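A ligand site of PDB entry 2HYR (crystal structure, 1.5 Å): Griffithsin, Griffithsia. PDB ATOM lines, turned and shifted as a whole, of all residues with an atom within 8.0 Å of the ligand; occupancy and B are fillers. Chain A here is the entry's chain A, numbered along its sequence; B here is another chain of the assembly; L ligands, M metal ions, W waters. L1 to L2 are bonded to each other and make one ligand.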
ATOM      1  N   TYR A  29      15.266   0.547  -8.654  1.00  0.00           N
ATOM      2  CA  TYR A  29      13.931   0.479  -9.219  1.00  0.00           C
ATOM      3  C   TYR A  29      13.436  -0.946  -9.103  1.00  0.00           C
ATOM      4  O   TYR A  29      14.174  -1.840  -8.623  1.00  0.00           O
ATOM      5  CB  TYR A  29      13.950   0.784 -10.756  1.00  0.00           C
ATOM      6  CG  TYR A  29      14.719   2.035 -11.130  1.00  0.00           C
ATOM      7  CD1 TYR A  29      14.488   3.205 -10.461  1.00  0.00           C
ATOM      8  CD2 TYR A  29      15.651   2.025 -12.106  1.00  0.00           C
ATOM      9  CE1 TYR A  29      15.213   4.370 -10.776  1.00  0.00           C
ATOM     10  CE2 TYR A  29      16.381   3.127 -12.429  1.00  0.00           C
ATOM     11  CZ  TYR A  29      16.140   4.306 -11.759  1.00  0.00           C
ATOM     12  OH  TYR A  29      16.865   5.455 -12.108  1.00  0.00           O
ATOM     13  N   LEU A  30      12.242  -1.198  -9.604  1.00  0.00           N
ATOM     14  CA  LEU A  30      11.811  -2.524  -9.948  1.00  0.00           C
ATOM     15  C   LEU A  30      12.316  -2.879 -11.333  1.00  0.00           C
ATOM     16  O   LEU A  30      11.991  -2.250 -12.354  1.00  0.00           O
ATOM     17  CB  LEU A  30      10.298  -2.677  -9.906  1.00  0.00           C
ATOM     18  CG  LEU A  30       9.797  -3.016  -8.500  1.00  0.00           C
ATOM     19  CD1 LEU A  30      10.302  -2.055  -7.462  1.00  0.00           C
ATOM     20  CD2 LEU A  30       8.295  -3.217  -8.372  1.00  0.00           C
ATOM     21  N   ASP A  31      13.221  -3.846 -11.354  1.00  0.00           N
ATOM     22  CA  ASP A  31      13.709  -4.406 -12.617  1.00  0.00           C
ATOM     23  C   ASP A  31      12.706  -5.301 -13.296  1.00  0.00           C
ATOM     24  O   ASP A  31      12.665  -5.349 -14.542  1.00  0.00           O
ATOM     25  CB  ASP A  31      14.993  -5.176 -12.378  1.00  0.00           C
ATOM     26  CG  ASP A  31      16.133  -4.278 -11.876  1.00  0.00           C
ATOM     27  OD1 ASP A  31      16.141  -3.980 -10.623  1.00  0.00           O
ATOM     28  OD2 ASP A  31      17.027  -3.946 -12.725  1.00  0.00           O
ATOM     29  N   GLY A  41      10.158  -8.155 -17.418  1.00  0.00           N
ATOM     30  CA  GLY A  41      11.175  -7.161 -17.184  1.00  0.00           C
ATOM     31  C   GLY A  41      12.544  -7.744 -17.305  1.00  0.00           C
ATOM     32  O   GLY A  41      12.745  -8.786 -17.977  1.00  0.00           O
ATOM     33  N   GLY A  42      13.506  -7.054 -16.729  1.00  0.00           N
ATOM     34  CA  GLY A  42      14.899  -7.343 -16.911  1.00  0.00           C
ATOM     35  C   GLY A  42      15.547  -8.305 -15.939  1.00  0.00           C
ATOM     36  O   GLY A  42      14.864  -8.859 -15.075  1.00  0.00           O
ATOM     37  N   ASP A  68       9.450   7.837 -14.145  1.00  0.00           N
ATOM     38  CA  ASP A  68       9.497   7.194 -15.456  1.00  0.00           C
ATOM     39  C   ASP A  68       9.342   5.640 -15.400  1.00  0.00           C
ATOM     40  O   ASP A  68       8.905   5.006 -16.328  1.00  0.00           O
ATOM     41  CB  ASP A  68      10.782   7.562 -16.166  1.00  0.00           C
ATOM     42  CG  ASP A  68      10.792   9.049 -16.625  1.00  0.00           C
ATOM     43  OD1 ASP A  68       9.770   9.747 -16.507  1.00  0.00           O
ATOM     44  OD2 ASP A  68      11.858   9.478 -17.104  1.00  0.00           O
ATOM     45  N   TYR A  69       9.741   5.051 -14.268  1.00  0.00           N
ATOM     46  CA  TYR A  69       9.639   3.636 -14.027  1.00  0.00           C
ATOM     47  C   TYR A  69       8.900   3.404 -12.728  1.00  0.00           C
ATOM     48  O   TYR A  69       8.485   4.361 -12.068  1.00  0.00           O
ATOM     49  CB  TYR A  69      11.051   3.018 -13.892  1.00  0.00           C
ATOM     50  CG  TYR A  69      12.060   3.431 -14.932  1.00  0.00           C
ATOM     51  CD1 TYR A  69      11.767   3.360 -16.275  1.00  0.00           C
ATOM     52  CD2 TYR A  69      13.310   3.837 -14.537  1.00  0.00           C
ATOM     53  CE1 TYR A  69      12.669   3.740 -17.222  1.00  0.00           C
ATOM     54  CE2 TYR A  69      14.263   4.185 -15.469  1.00  0.00           C
ATOM     55  CZ  TYR A  69      13.929   4.136 -16.829  1.00  0.00           C
ATOM     56  OH  TYR A  69      14.885   4.501 -17.807  1.00  0.00           O
ATOM     57  N   SER A 107       3.983  -2.549 -18.368  1.00  0.00           N
ATOM     58  CA  SER A 107       4.901  -2.491 -19.469  1.00  0.00           C
ATOM     59  C   SER A 107       6.305  -2.621 -18.907  1.00  0.00           C
ATOM     60  O   SER A 107       6.630  -2.030 -17.845  1.00  0.00           O
ATOM     61  CB  SER A 107       4.726  -1.153 -20.188  1.00  0.00           C
ATOM     62  OG  SER A 107       5.483  -1.170 -21.385  1.00  0.00           O
ATOM     63  N   ALA A 108       7.174  -3.297 -19.613  1.00  0.00           N
ATOM     64  CA  ALA A 108       8.501  -3.555 -19.096  1.00  0.00           C
ATOM     65  C   ALA A 108       9.482  -3.671 -20.202  1.00  0.00           C
ATOM     66  O   ALA A 108       9.172  -4.179 -21.277  1.00  0.00           O
ATOM     67  CB  ALA A 108       8.519  -4.828 -18.275  1.00  0.00           C
ATOM     68  N   GLY A 109      10.685  -3.189 -19.936  1.00  0.00           N
ATOM     69  CA  GLY A 109      11.857  -3.403 -20.800  1.00  0.00           C
ATOM     70  C   GLY A 109      12.989  -3.988 -19.962  1.00  0.00           C
ATOM     71  O   GLY A 109      12.807  -5.000 -19.343  1.00  0.00           O
ATOM     72  N   ASP A 110      14.082  -3.250 -19.863  1.00  0.00           N
ATOM     73  CA  ASP A 110      15.148  -3.598 -18.901  1.00  0.00           C
ATOM     74  C   ASP A 110      14.703  -3.405 -17.475  1.00  0.00           C
ATOM     75  O   ASP A 110      15.166  -4.086 -16.578  1.00  0.00           O
ATOM     76  CB  ASP A 110      16.363  -2.794 -19.267  1.00  0.00           C
ATOM     77  CG  ASP A 110      16.960  -3.318 -20.636  1.00  0.00           C
ATOM     78  OD1 ASP A 110      17.332  -4.526 -20.680  1.00  0.00           O
ATOM     79  OD2 ASP A 110      16.893  -2.628 -21.666  1.00  0.00           O
ATOM     80  N   TYR A 111      13.778  -2.497 -17.265  1.00  0.00           N
ATOM     81  CA  TYR A 111      13.099  -2.256 -15.997  1.00  0.00           C
ATOM     82  C   TYR A 111      11.613  -2.338 -16.117  1.00  0.00           C
ATOM     83  O   TYR A 111      11.055  -2.443 -17.209  1.00  0.00           O
ATOM     84  CB  TYR A 111      13.474  -0.863 -15.416  1.00  0.00           C
ATOM     85  CG  TYR A 111      14.934  -0.533 -15.377  1.00  0.00           C
ATOM     86  CD1 TYR A 111      15.852  -1.386 -14.768  1.00  0.00           C
ATOM     87  CD2 TYR A 111      15.394   0.658 -15.935  1.00  0.00           C
ATOM     88  CE1 TYR A 111      17.214  -1.080 -14.744  1.00  0.00           C
ATOM     89  CE2 TYR A 111      16.701   0.978 -15.879  1.00  0.00           C
ATOM     90  CZ  TYR A 111      17.608   0.116 -15.289  1.00  0.00           C
ATOM     91  OH  TYR A 111      18.912   0.596 -15.310  1.00  0.00           O
ATOM     92  N   LEU A 112      10.930  -2.255 -14.972  1.00  0.00           N
ATOM     93  CA  LEU A 112       9.483  -2.192 -14.989  1.00  0.00           C
ATOM     94  C   LEU A 112       9.073  -0.790 -15.190  1.00  0.00           C
ATOM     95  O   LEU A 112       9.148   0.009 -14.263  1.00  0.00           O
ATOM     96  CB  LEU A 112       8.967  -2.707 -13.638  1.00  0.00           C
ATOM     97  CG  LEU A 112       7.490  -2.898 -13.563  1.00  0.00           C
ATOM     98  CD1 LEU A 112       6.851  -3.758 -14.633  1.00  0.00           C
ATOM     99  CD2 LEU A 112       7.158  -3.484 -12.193  1.00  0.00           C
ATOM    100  N   ASP A 113       8.668  -0.423 -16.402  1.00  0.00           N
ATOM    101  CA  ASP A 113       8.280   0.944 -16.719  1.00  0.00           C
ATOM    102  C   ASP A 113       6.980   1.391 -16.067  1.00  0.00           C
ATOM    103  O   ASP A 113       6.839   2.521 -15.607  1.00  0.00           O
ATOM    104  CB  ASP A 113       8.159   1.112 -18.225  1.00  0.00           C
ATOM    105  CG  ASP A 113       9.486   0.952 -18.931  1.00  0.00           C
ATOM    106  OD1 ASP A 113       9.895  -0.245 -19.129  1.00  0.00           O
ATOM    107  OD2 ASP A 113      10.125   2.002 -19.224  1.00  0.00           O
ATOM    108  N   SER A 114       6.002   0.510 -16.089  1.00  0.00           N
ATOM    109  CA  SER A 114       4.671   0.826 -15.594  1.00  0.00           C
ATOM    110  C   SER A 114       3.915  -0.354 -15.132  1.00  0.00           C
ATOM    111  O   SER A 114       4.211  -1.492 -15.503  1.00  0.00           O
ATOM    112  CB  SER A 114       3.883   1.599 -16.594  1.00  0.00           C
ATOM    113  OG  SER A 114       3.628   0.757 -17.716  1.00  0.00           O
ATOM    114  N   GLY B  10       5.825   5.232 -16.300  1.00  0.00           N
ATOM    115  CA  GLY B  10       6.089   5.970 -17.494  1.00  0.00           C
ATOM    116  C   GLY B  10       5.569   5.306 -18.709  1.00  0.00           C
ATOM    117  O   GLY B  10       4.763   4.372 -18.621  1.00  0.00           O
ATOM    118  N   SER B  11       6.008   5.826 -19.879  1.00  0.00           N
ATOM    119  CA  SER B  11       5.520   5.415 -21.157  1.00  0.00           C
ATOM    120  C   SER B  11       6.382   4.352 -21.882  1.00  0.00           C
ATOM    121  O   SER B  11       5.958   3.860 -22.920  1.00  0.00           O
ATOM    122  CB  SER B  11       5.469   6.627 -22.073  1.00  0.00           C
ATOM    123  OG  SER B  11       6.664   7.349 -22.020  1.00  0.00           O
ATOM    124  N   GLY B  12       7.540   3.988 -21.331  1.00  0.00           N
ATOM    125  CA  GLY B  12       8.429   3.020 -21.954  1.00  0.00           C
ATOM    126  C   GLY B  12       8.020   1.580 -21.843  1.00  0.00           C
ATOM    127  O   GLY B  12       7.029   1.223 -21.186  1.00  0.00           O
ATOM    128  N   GLY B  13       8.835   0.727 -22.471  1.00  0.00           N
ATOM    129  CA  GLY B  13       8.684  -0.685 -22.326  1.00  0.00           C
ATOM    130  C   GLY B  13       7.706  -1.317 -23.245  1.00  0.00           C
ATOM    131  O   GLY B  13       6.957  -0.610 -23.908  1.00  0.00           O
ATOM    132  N   SER B  14       7.653  -2.627 -23.191  1.00  0.00           N
ATOM    133  CA  SER B  14       6.754  -3.456 -23.926  1.00  0.00           C
ATOM    134  C   SER B  14       5.591  -3.899 -23.067  1.00  0.00           C
ATOM    135  O   SER B  14       5.814  -4.430 -21.941  1.00  0.00           O
ATOM    136  CB  SER B  14       7.474  -4.686 -24.444  1.00  0.00           C
ATOM    137  OG  SER B  14       8.621  -4.421 -25.137  1.00  0.00           O
HETATM  138  C1  LIG L   1      18.558   0.536 -24.974  1.00  0.00           C
HETATM  139  C2  LIG L   1      17.057   0.464 -24.754  1.00  0.00           C
HETATM  140  C3  LIG L   1      16.724   0.413 -23.262  1.00  0.00           C
HETATM  141  C4  LIG L   1      17.494   1.479 -22.494  1.00  0.00           C
HETATM  142  C5  LIG L   1      17.234   1.359 -20.993  1.00  0.00           C
HETATM  143  C6  LIG L   1      19.194   1.610 -24.101  1.00  0.00           C
HETATM  144  O1  LIG L   1      20.589   1.604 -24.262  1.00  0.00           O
HETATM  145  O2  LIG L   1      18.822   0.820 -26.329  1.00  0.00           O
HETATM  146  O3  LIG L   1      16.532  -0.676 -25.398  1.00  0.00           O
HETATM  147  O4  LIG L   1      15.338   0.622 -23.091  1.00  0.00           O
HETATM  148  O5  LIG L   1      18.870   1.348 -22.750  1.00  0.00           O
HETATM  149  O6  LIG L   1      17.130   2.651 -20.426  1.00  0.00           O
HETATM  150  C1  LG2 L   2      14.491  -0.530 -22.785  1.00  0.00           C
HETATM  151  C2  LG2 L   2      13.221  -0.373 -23.607  1.00  0.00           C
HETATM  152  C3  LG2 L   2      12.501   0.908 -23.209  1.00  0.00           C
HETATM  153  C4  LG2 L   2      12.282   0.925 -21.695  1.00  0.00           C
HETATM  154  C5  LG2 L   2      13.583   0.648 -20.958  1.00  0.00           C
HETATM  155  C6  LG2 L   2      13.346   0.552 -19.462  1.00  0.00           C
HETATM  156  O1  LG2 L   2      13.547  -0.320 -24.982  1.00  0.00           O
HETATM  157  O2  LG2 L   2      11.256   0.986 -23.877  1.00  0.00           O
HETATM  158  O3  LG2 L   2      11.778   2.178 -21.314  1.00  0.00           O
HETATM  159  O4  LG2 L   2      14.151  -0.565 -21.415  1.00  0.00           O
HETATM  160  O5  LG2 L   2      12.548  -0.581 -19.180  1.00  0.00           O
HETATM  161 MG    MG M   1      15.067  -4.481 -25.112  1.00  0.00          MG
HETATM  162  O   HOH W   1      11.191   4.239 -24.581  1.00  0.00           O
HETATM  163  O   HOH W   2      13.768  -3.030 -25.923  1.00  0.00           O
HETATM  164  O   HOH W   3      14.345   1.721 -26.286  1.00  0.00           O
HETATM  165  O   HOH W   4      16.430  -3.131 -24.471  1.00  0.00           O
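OD2 of Asp 113 is in hydrogen-bond range of O3 of LG2 L2 (2.7 Å). O2 of LG2 L2 lies within hydrogen-bond range of N of Gly 13 of chain B (2.8 Å). The backbone NH (N) of Tyr 111 sits at hydrogen-bond distance from an oxygen (O5) of LG2 L2 (3.0 Å). The backbone carbonyl oxygen (O) of Tyr 111 sits at hydrogen-bond distance from an oxygen (O5) of LG2 L2, 3.1 Å away. An oxygen (O4) of LG2 L2 lies within hydrogen-bond range of the backbone NH of Asp 110, at 3.1 Å. The backbone NH (N) of Gly 109 lies within hydrogen-bond range of an oxygen (O5) of LG2 L2, at 3.3 Å.
The backbone NH of Gly 109 lies within hydrogen-bond range of the side-chain carboxylate of Asp 113 (3.2 Å). The backbone carbonyl oxygen (O) of Ser 107 is in hydrogen-bond range of the backbone NH (N) of Asp 113. The backbone NH (N) of Gly 10 of chain B is in hydrogen-bond range of the backbone carbonyl oxygen (O) of Asp 113 (3.0 Å). O of Gly 13 of chain B lies close to OG of Ser 107. N of Gly 42 sits close to O of Asp 110, 3.4 Å away. O of Gly 109 lies within hydrogen-bond range of N of Gly 42, at 3.4 Å. The backbone carbonyl oxygen (O) of Gly 12 of chain B is in hydrogen-bond range of the side-chain hydroxyl (OG) of Ser 107 (2.9 Å).
OH of Tyr 69 touches O6 of LIG L1, 3.9 Å away. CA of Gly 12 of chain B touches O3 of LG2 L2 (3.5 Å). Hydrophobic or aromatic side chains that line the ligand: Tyr 69 and Tyr 111. Of the 20 residues printed, 7 come within 4 Å of the ligand.
Water W4 lies within hydrogen-bond range of O3 of LIG L1 (2.6 Å) and OD2 of Asp 110 (2.9 Å).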
